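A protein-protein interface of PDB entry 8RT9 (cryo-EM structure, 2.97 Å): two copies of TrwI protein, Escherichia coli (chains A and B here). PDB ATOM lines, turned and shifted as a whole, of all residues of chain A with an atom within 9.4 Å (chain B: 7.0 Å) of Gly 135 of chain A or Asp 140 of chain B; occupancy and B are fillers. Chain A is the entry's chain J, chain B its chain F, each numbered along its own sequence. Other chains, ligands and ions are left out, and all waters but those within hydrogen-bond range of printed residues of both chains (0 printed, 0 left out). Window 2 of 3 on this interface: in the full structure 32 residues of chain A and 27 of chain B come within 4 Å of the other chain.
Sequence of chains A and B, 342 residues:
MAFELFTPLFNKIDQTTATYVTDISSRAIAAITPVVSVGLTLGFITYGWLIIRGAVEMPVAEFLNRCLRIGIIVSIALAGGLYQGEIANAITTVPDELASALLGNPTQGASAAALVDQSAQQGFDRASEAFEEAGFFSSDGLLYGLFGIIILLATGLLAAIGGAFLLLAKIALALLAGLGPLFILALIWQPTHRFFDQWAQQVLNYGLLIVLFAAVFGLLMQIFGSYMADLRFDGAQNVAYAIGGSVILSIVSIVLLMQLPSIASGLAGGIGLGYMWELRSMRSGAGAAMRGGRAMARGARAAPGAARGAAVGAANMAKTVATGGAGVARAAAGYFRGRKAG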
ATOM      1  N   ALA A 127      29.053  13.500 -26.965  1.00  0.00           N
ATOM      2  CA  ALA A 127      28.520  14.748 -26.427  1.00  0.00           C
ATOM      3  C   ALA A 127      27.623  15.449 -27.439  1.00  0.00           C
ATOM      4  O   ALA A 127      26.590  16.023 -27.078  1.00  0.00           O
ATOM      5  CB  ALA A 127      29.661  15.667 -25.999  1.00  0.00           C
ATOM      6  N   SER A 128      28.010  15.422 -28.713  1.00  0.00           N
ATOM      7  CA  SER A 128      27.204  16.039 -29.758  1.00  0.00           C
ATOM      8  C   SER A 128      25.868  15.333 -29.915  1.00  0.00           C
ATOM      9  O   SER A 128      24.842  15.979 -30.146  1.00  0.00           O
ATOM     10  CB  SER A 128      27.969  16.028 -31.076  1.00  0.00           C
ATOM     11  OG  SER A 128      27.081  16.137 -32.169  1.00  0.00           O
ATOM     12  N   GLU A 129      25.862  14.008 -29.807  1.00  0.00           N
ATOM     13  CA  GLU A 129      24.602  13.278 -29.853  1.00  0.00           C
ATOM     14  C   GLU A 129      23.720  13.642 -28.670  1.00  0.00           C
ATOM     15  O   GLU A 129      22.497  13.767 -28.810  1.00  0.00           O
ATOM     16  CB  GLU A 129      24.871  11.778 -29.888  1.00  0.00           C
ATOM     17  CG  GLU A 129      25.540  11.323 -31.166  1.00  0.00           C
ATOM     18  CD  GLU A 129      25.820   9.840 -31.179  1.00  0.00           C
ATOM     19  OE1 GLU A 129      25.606   9.185 -30.139  1.00  0.00           O
ATOM     20  OE2 GLU A 129      26.256   9.328 -32.229  1.00  0.00           O
ATOM     21  N   ALA A 130      24.322  13.815 -27.495  1.00  0.00           N
ATOM     22  CA  ALA A 130      23.549  14.268 -26.343  1.00  0.00           C
ATOM     23  C   ALA A 130      22.948  15.645 -26.592  1.00  0.00           C
ATOM     24  O   ALA A 130      21.791  15.901 -26.241  1.00  0.00           O
ATOM     25  CB  ALA A 130      24.425  14.283 -25.094  1.00  0.00           C
ATOM     26  N   PHE A 131      23.722  16.546 -27.195  1.00  0.00           N
ATOM     27  CA  PHE A 131      23.204  17.874 -27.511  1.00  0.00           C
ATOM     28  C   PHE A 131      22.069  17.793 -28.518  1.00  0.00           C
ATOM     29  O   PHE A 131      21.100  18.554 -28.439  1.00  0.00           O
ATOM     30  CB  PHE A 131      24.322  18.760 -28.050  1.00  0.00           C
ATOM     31  CG  PHE A 131      25.371  19.086 -27.044  1.00  0.00           C
ATOM     32  CD1 PHE A 131      25.077  19.092 -25.700  1.00  0.00           C
ATOM     33  CD2 PHE A 131      26.654  19.382 -27.442  1.00  0.00           C
ATOM     34  CE1 PHE A 131      26.043  19.389 -24.775  1.00  0.00           C
ATOM     35  CE2 PHE A 131      27.621  19.679 -26.522  1.00  0.00           C
ATOM     36  CZ  PHE A 131      27.317  19.681 -25.187  1.00  0.00           C
ATOM     37  N   GLU A 132      22.184  16.892 -29.489  1.00  0.00           N
ATOM     38  CA  GLU A 132      21.116  16.698 -30.460  1.00  0.00           C
ATOM     39  C   GLU A 132      19.841  16.224 -29.779  1.00  0.00           C
ATOM     40  O   GLU A 132      18.743  16.706 -30.082  1.00  0.00           O
ATOM     41  CB  GLU A 132      21.569  15.697 -31.516  1.00  0.00           C
ATOM     42  CG  GLU A 132      20.874  15.822 -32.840  1.00  0.00           C
ATOM     43  CD  GLU A 132      21.204  14.690 -33.774  1.00  0.00           C
ATOM     44  OE1 GLU A 132      22.324  14.153 -33.679  1.00  0.00           O
ATOM     45  OE2 GLU A 132      20.349  14.340 -34.613  1.00  0.00           O
ATOM     46  N   GLU A 133      19.971  15.285 -28.844  1.00  0.00           N
ATOM     47  CA  GLU A 133      18.807  14.839 -28.086  1.00  0.00           C
ATOM     48  C   GLU A 133      18.216  15.979 -27.277  1.00  0.00           C
ATOM     49  O   GLU A 133      16.991  16.091 -27.147  1.00  0.00           O
ATOM     50  CB  GLU A 133      19.183  13.677 -27.176  1.00  0.00           C
ATOM     51  CG  GLU A 133      19.386  12.376 -27.905  1.00  0.00           C
ATOM     52  CD  GLU A 133      18.127  11.905 -28.594  1.00  0.00           C
ATOM     53  OE1 GLU A 133      17.033  12.084 -28.021  1.00  0.00           O
ATOM     54  OE2 GLU A 133      18.227  11.360 -29.712  1.00  0.00           O
ATOM     55  N   ALA A 134      19.071  16.828 -26.712  1.00  0.00           N
ATOM     56  CA  ALA A 134      18.585  18.007 -26.005  1.00  0.00           C
ATOM     57  C   ALA A 134      17.807  18.917 -26.939  1.00  0.00           C
ATOM     58  O   ALA A 134      16.808  19.522 -26.543  1.00  0.00           O
ATOM     59  CB  ALA A 134      19.753  18.763 -25.378  1.00  0.00           C
ATOM     60  N   GLY A 135      18.267  19.040 -28.179  1.00  0.00           N
ATOM     61  CA  GLY A 135      17.540  19.836 -29.151  1.00  0.00           C
ATOM     62  C   GLY A 135      16.188  19.245 -29.492  1.00  0.00           C
ATOM     63  O   GLY A 135      15.224  19.976 -29.729  1.00  0.00           O
ATOM     64  N   PHE A 136      16.097  17.915 -29.527  1.00  0.00           N
ATOM     65  CA  PHE A 136      14.824  17.276 -29.850  1.00  0.00           C
ATOM     66  C   PHE A 136      13.760  17.599 -28.811  1.00  0.00           C
ATOM     67  O   PHE A 136      12.662  18.051 -29.150  1.00  0.00           O
ATOM     68  CB  PHE A 136      15.008  15.767 -29.967  1.00  0.00           C
ATOM     69  CG  PHE A 136      13.730  15.021 -30.183  1.00  0.00           C
ATOM     70  CD1 PHE A 136      13.112  15.029 -31.410  1.00  0.00           C
ATOM     71  CD2 PHE A 136      13.147  14.315 -29.156  1.00  0.00           C
ATOM     72  CE1 PHE A 136      11.940  14.349 -31.609  1.00  0.00           C
ATOM     73  CE2 PHE A 136      11.974  13.632 -29.355  1.00  0.00           C
ATOM     74  CZ  PHE A 136      11.373  13.650 -30.580  1.00  0.00           C
ATOM     75  N   PHE A 137      14.062  17.372 -27.537  1.00  0.00           N
ATOM     76  CA  PHE A 137      13.148  17.715 -26.452  1.00  0.00           C
ATOM     77  C   PHE A 137      13.354  19.183 -26.119  1.00  0.00           C
ATOM     78  O   PHE A 137      14.329  19.545 -25.459  1.00  0.00           O
ATOM     79  CB  PHE A 137      13.405  16.846 -25.229  1.00  0.00           C
ATOM     80  CG  PHE A 137      13.377  15.374 -25.504  1.00  0.00           C
ATOM     81  CD1 PHE A 137      12.179  14.706 -25.646  1.00  0.00           C
ATOM     82  CD2 PHE A 137      14.547  14.654 -25.604  1.00  0.00           C
ATOM     83  CE1 PHE A 137      12.155  13.354 -25.892  1.00  0.00           C
ATOM     84  CE2 PHE A 137      14.524  13.305 -25.851  1.00  0.00           C
ATOM     85  CZ  PHE A 137      13.329  12.656 -25.995  1.00  0.00           C
ATOM     86  N   SER A 138      12.442  20.042 -26.574  1.00  0.00           N
ATOM     87  CA  SER A 138      12.602  21.477 -26.372  1.00  0.00           C
ATOM     88  C   SER A 138      12.723  21.796 -24.890  1.00  0.00           C
ATOM     89  O   SER A 138      13.790  22.203 -24.422  1.00  0.00           O
ATOM     90  CB  SER A 138      11.428  22.238 -26.989  1.00  0.00           C
ATOM     91  OG  SER A 138      11.539  23.630 -26.756  1.00  0.00           O
ATOM     92  N   SER A 139      11.651  21.591 -24.141  1.00  0.00           N
ATOM     93  CA  SER A 139      11.748  21.497 -22.697  1.00  0.00           C
ATOM     94  C   SER A 139      11.886  20.029 -22.316  1.00  0.00           C
ATOM     95  O   SER A 139      11.657  19.131 -23.129  1.00  0.00           O
ATOM     96  CB  SER A 139      10.531  22.131 -22.030  1.00  0.00           C
ATOM     97  OG  SER A 139      10.449  23.510 -22.340  1.00  0.00           O
ATOM     98  N   ASP A 140      12.267  19.784 -21.066  1.00  0.00           N
ATOM     99  CA  ASP A 140      12.646  18.443 -20.625  1.00  0.00           C
ATOM    100  C   ASP A 140      13.790  17.899 -21.471  1.00  0.00           C
ATOM    101  O   ASP A 140      13.872  16.698 -21.734  1.00  0.00           O
ATOM    102  CB  ASP A 140      11.456  17.479 -20.653  1.00  0.00           C
ATOM    103  CG  ASP A 140      11.666  16.263 -19.768  1.00  0.00           C
ATOM    104  OD1 ASP A 140      12.723  16.179 -19.109  1.00  0.00           O
ATOM    105  OD2 ASP A 140      10.771  15.393 -19.731  1.00  0.00           O
ATOM    106  N   GLY A 141      14.675  18.784 -21.910  1.00  0.00           N
ATOM    107  CA  GLY A 141      15.770  18.382 -22.761  1.00  0.00           C
ATOM    108  C   GLY A 141      17.106  18.851 -22.239  1.00  0.00           C
ATOM    109  O   GLY A 141      18.152  18.377 -22.688  1.00  0.00           O
ATOM    110  N   LEU A 142      17.091  19.778 -21.282  1.00  0.00           N
ATOM    111  CA  LEU A 142      18.345  20.266 -20.732  1.00  0.00           C
ATOM    112  C   LEU A 142      19.064  19.206 -19.915  1.00  0.00           C
ATOM    113  O   LEU A 142      20.260  19.353 -19.646  1.00  0.00           O
ATOM    114  CB  LEU A 142      18.109  21.511 -19.888  1.00  0.00           C
ATOM    115  CG  LEU A 142      19.361  22.374 -19.738  1.00  0.00           C
ATOM    116  CD1 LEU A 142      19.948  22.701 -21.103  1.00  0.00           C
ATOM    117  CD2 LEU A 142      19.051  23.637 -18.980  1.00  0.00           C
ATOM    118  N   LEU A 143      18.368  18.143 -19.520  1.00  0.00           N
ATOM    119  CA  LEU A 143      19.052  17.008 -18.917  1.00  0.00           C
ATOM    120  C   LEU A 143      20.073  16.422 -19.880  1.00  0.00           C
ATOM    121  O   LEU A 143      21.205  16.104 -19.493  1.00  0.00           O
ATOM    122  CB  LEU A 143      18.030  15.955 -18.503  1.00  0.00           C
ATOM    123  CG  LEU A 143      18.548  14.783 -17.683  1.00  0.00           C
ATOM    124  CD1 LEU A 143      19.451  15.283 -16.578  1.00  0.00           C
ATOM    125  CD2 LEU A 143      17.392  13.993 -17.117  1.00  0.00           C
ATOM    126  N   TYR A 144      19.693  16.283 -21.149  1.00  0.00           N
ATOM    127  CA  TYR A 144      20.635  15.811 -22.151  1.00  0.00           C
ATOM    128  C   TYR A 144      21.746  16.820 -22.382  1.00  0.00           C
ATOM    129  O   TYR A 144      22.880  16.435 -22.682  1.00  0.00           O
ATOM    130  CB  TYR A 144      19.903  15.498 -23.449  1.00  0.00           C
ATOM    131  CG  TYR A 144      18.876  14.407 -23.303  1.00  0.00           C
ATOM    132  CD1 TYR A 144      17.582  14.695 -22.921  1.00  0.00           C
ATOM    133  CD2 TYR A 144      19.207  13.088 -23.539  1.00  0.00           C
ATOM    134  CE1 TYR A 144      16.646  13.704 -22.785  1.00  0.00           C
ATOM    135  CE2 TYR A 144      18.278  12.091 -23.405  1.00  0.00           C
ATOM    136  CZ  TYR A 144      16.999  12.404 -23.028  1.00  0.00           C
ATOM    137  OH  TYR A 144      16.065  11.410 -22.891  1.00  0.00           O
ATOM    138  N   GLY A 145      21.450  18.108 -22.229  1.00  0.00           N
ATOM    139  CA  GLY A 145      22.503  19.102 -22.288  1.00  0.00           C
ATOM    140  C   GLY A 145      23.524  18.922 -21.185  1.00  0.00           C
ATOM    141  O   GLY A 145      24.728  19.021 -21.420  1.00  0.00           O
ATOM    142  N   GLU B 133      22.254  33.506 -28.648  1.00  0.00           N
ATOM    143  CA  GLU B 133      21.509  32.355 -29.146  1.00  0.00           C
ATOM    144  C   GLU B 133      20.601  31.788 -28.069  1.00  0.00           C
ATOM    145  O   GLU B 133      19.484  31.345 -28.355  1.00  0.00           O
ATOM    146  CB  GLU B 133      22.467  31.284 -29.653  1.00  0.00           C
ATOM    147  CG  GLU B 133      23.098  31.611 -30.980  1.00  0.00           C
ATOM    148  CD  GLU B 133      22.076  31.713 -32.088  1.00  0.00           C
ATOM    149  OE1 GLU B 133      21.106  30.928 -32.075  1.00  0.00           O
ATOM    150  OE2 GLU B 133      22.240  32.579 -32.973  1.00  0.00           O
ATOM    151  N   ALA B 134      21.069  31.783 -26.821  1.00  0.00           N
ATOM    152  CA  ALA B 134      20.214  31.367 -25.716  1.00  0.00           C
ATOM    153  C   ALA B 134      19.007  32.280 -25.594  1.00  0.00           C
ATOM    154  O   ALA B 134      17.897  31.825 -25.305  1.00  0.00           O
ATOM    155  CB  ALA B 134      21.007  31.356 -24.413  1.00  0.00           C
ATOM    156  N   PHE B 137      16.202  31.313 -28.402  1.00  0.00           N
ATOM    157  CA  PHE B 137      15.367  30.186 -27.995  1.00  0.00           C
ATOM    158  C   PHE B 137      14.966  30.405 -26.544  1.00  0.00           C
ATOM    159  O   PHE B 137      15.764  30.181 -25.633  1.00  0.00           O
ATOM    160  CB  PHE B 137      16.116  28.871 -28.158  1.00  0.00           C
ATOM    161  CG  PHE B 137      16.697  28.662 -29.523  1.00  0.00           C
ATOM    162  CD1 PHE B 137      15.899  28.277 -30.578  1.00  0.00           C
ATOM    163  CD2 PHE B 137      18.045  28.836 -29.747  1.00  0.00           C
ATOM    164  CE1 PHE B 137      16.436  28.082 -31.829  1.00  0.00           C
ATOM    165  CE2 PHE B 137      18.582  28.642 -30.996  1.00  0.00           C
ATOM    166  CZ  PHE B 137      17.780  28.265 -32.035  1.00  0.00           C
ATOM    167  N   SER B 138      13.728  30.844 -26.317  1.00  0.00           N
ATOM    168  CA  SER B 138      13.282  31.174 -24.969  1.00  0.00           C
ATOM    169  C   SER B 138      13.436  29.974 -24.046  1.00  0.00           C
ATOM    170  O   SER B 138      14.266  29.986 -23.134  1.00  0.00           O
ATOM    171  CB  SER B 138      11.829  31.650 -24.988  1.00  0.00           C
ATOM    172  OG  SER B 138      11.362  31.921 -23.678  1.00  0.00           O
ATOM    173  N   SER B 139      12.660  28.930 -24.288  1.00  0.00           N
ATOM    174  CA  SER B 139      12.977  27.620 -23.755  1.00  0.00           C
ATOM    175  C   SER B 139      13.784  26.860 -24.800  1.00  0.00           C
ATOM    176  O   SER B 139      13.878  27.267 -25.959  1.00  0.00           O
ATOM    177  CB  SER B 139      11.705  26.865 -23.380  1.00  0.00           C
ATOM    178  OG  SER B 139      11.017  27.525 -22.334  1.00  0.00           O
ATOM    179  N   ASP B 140      14.379  25.747 -24.381  1.00  0.00           N
ATOM    180  CA  ASP B 140      15.338  25.026 -25.215  1.00  0.00           C
ATOM    181  C   ASP B 140      16.494  25.932 -25.618  1.00  0.00           C
ATOM    182  O   ASP B 140      17.046  25.810 -26.714  1.00  0.00           O
ATOM    183  CB  ASP B 140      14.673  24.427 -26.458  1.00  0.00           C
ATOM    184  CG  ASP B 140      15.483  23.297 -27.067  1.00  0.00           C
ATOM    185  OD1 ASP B 140      16.545  22.954 -26.508  1.00  0.00           O
ATOM    186  OD2 ASP B 140      15.053  22.750 -28.105  1.00  0.00           O
ATOM    187  N   GLY B 141      16.860  26.855 -24.740  1.00  0.00           N
ATOM    188  CA  GLY B 141      17.915  27.792 -25.044  1.00  0.00           C
ATOM    189  C   GLY B 141      18.984  27.830 -23.978  1.00  0.00           C
ATOM    190  O   GLY B 141      20.076  28.352 -24.210  1.00  0.00           O
ATOM    191  N   LEU B 142      18.690  27.268 -22.806  1.00  0.00           N
ATOM    192  CA  LEU B 142      19.675  27.277 -21.736  1.00  0.00           C
ATOM    193  C   LEU B 142      20.865  26.383 -22.043  1.00  0.00           C
ATOM    194  O   LEU B 142      21.902  26.504 -21.383  1.00  0.00           O
ATOM    195  CB  LEU B 142      19.032  26.865 -20.417  1.00  0.00           C
ATOM    196  CG  LEU B 142      19.813  27.346 -19.195  1.00  0.00           C
ATOM    197  CD1 LEU B 142      20.046  28.847 -19.271  1.00  0.00           C
ATOM    198  CD2 LEU B 142      19.090  26.986 -17.924  1.00  0.00           C
ATOM    199  N   LEU B 143      20.746  25.497 -23.028  1.00  0.00           N
ATOM    200  CA  LEU B 143      21.919  24.778 -23.505  1.00  0.00           C
ATOM    201  C   LEU B 143      22.961  25.748 -24.040  1.00  0.00           C
ATOM    202  O   LEU B 143      24.160  25.608 -23.767  1.00  0.00           O
ATOM    203  CB  LEU B 143      21.507  23.779 -24.581  1.00  0.00           C
ATOM    204  CG  LEU B 143      22.581  22.816 -25.065  1.00  0.00           C
ATOM    205  CD1 LEU B 143      23.326  22.230 -23.887  1.00  0.00           C
ATOM    206  CD2 LEU B 143      21.961  21.726 -25.907  1.00  0.00           C
ATOM    207  N   TYR B 144      22.517  26.749 -24.797  1.00  0.00           N
ATOM    208  CA  TYR B 144      23.432  27.773 -25.273  1.00  0.00           C
ATOM    209  C   TYR B 144      23.965  28.612 -24.125  1.00  0.00           C
ATOM    210  O   TYR B 144      25.108  29.079 -24.178  1.00  0.00           O
ATOM    211  CB  TYR B 144      22.740  28.646 -26.309  1.00  0.00           C
ATOM    212  CG  TYR B 144      22.305  27.882 -27.529  1.00  0.00           C
ATOM    213  CD1 TYR B 144      21.101  27.205 -27.554  1.00  0.00           C
ATOM    214  CD2 TYR B 144      23.101  27.832 -28.656  1.00  0.00           C
ATOM    215  CE1 TYR B 144      20.703  26.506 -28.663  1.00  0.00           C
ATOM    216  CE2 TYR B 144      22.711  27.137 -29.770  1.00  0.00           C
ATOM    217  CZ  TYR B 144      21.511  26.475 -29.767  1.00  0.00           C
ATOM    218  OH  TYR B 144      21.117  25.777 -30.880  1.00  0.00           O
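Ala 134 of chain A touches Asp 140 of chain B, but with the chains exchanged Asp 140 of chain A does not touch Ala 134 of chain B (14.0 Å).
Ser 138 of chain A touches Asp 140 of chain B, but with the chains exchanged Asp 140 of chain A does not touch Ser 138 of chain B (10.6 Å).
Leu 142 of chain A touches its own counterpart, Leu 142 of chain B.
Leu 142 of chain A touches Leu 143 of chain B, but with the chains exchanged Leu 143 of chain A does not touch Leu 142 of chain B (8.8 Å).
Of the 8 pairs that touch across the chains among the printed residues, 2 have their exchanged pair printed and touching as well.
Leu 143 of chain B touches Ala 134 of chain A (CD2 to CB, 3.7 Å).
Ser 138 of chain A touches Asp 140 of chain B (O to CB, 3.1 Å).
CB of Ser 139 of chain B touches OG of Ser 139 of chain A, at 3.7 Å.
Leu 142 of chain B touches Leu 142 of chain A (CD2 to CD2, 3.5 Å).
N of Leu 143 of chain B touches CD1 of Leu 142 of chain A, 3.5 Å away.
Gly 145 of chain A touches Leu 143 of chain B.
Glu 132 of chain A touches none of the printed residues of chain B.
Of chain B, only Asp 140 (3.2 Å) comes within 4 Å of Gly 135 of chain A.
Of the printed residues of chain B, Ser 138 of chain A touches Asp 140 (3.1 Å).
Gly 141 of chain A touches none of the printed residues of chain B.
Printed residues of chain B within 4 Å of Leu 142 of chain A: Leu 142 (3.5 Å) and Leu 143 (3.5 Å).
Ser 139 of chain B touches just one residue of chain A: Ser 139 (3.7 Å).
Printed residues of chain A within 4 Å of Asp 140 of chain B: Ala 134 (3.4 Å), Gly 135 (3.2 Å) and Ser 138 (3.1 Å).
The nearest residue of chain B that does not touch Gly 135 of chain A is Leu 143 of chain B (5.1 Å).
The nearest residue of chain A that does not touch Asp 140 of chain B is Phe 137 of chain A (4.2 Å).
The nearest printed residue of chain B that does not touch Ser 138 of chain A is Ser 139 of chain B (4.4 Å).
OD1 of Asp 140 of chain B sits close to O of Ala 134 of chain A (3.4 Å).
The backbone carbonyl oxygen (O) of Gly 135 of chain A lies close to the side-chain carboxylate (OD2) of Asp 140 of chain B (3.2 Å).
Printed residues of chain B that touch a printed residue of chain A: Ser 139, Asp 140, Leu 142 and Leu 143.
Hydrophobic or aromatic side chains of chain B that line the printed part of chain A: Leu 142 and Leu 143.
Among the printed residues, no Asp or Glu carboxylate lies within 4 Å of a Lys or Arg side-chain nitrogen of the other chain.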
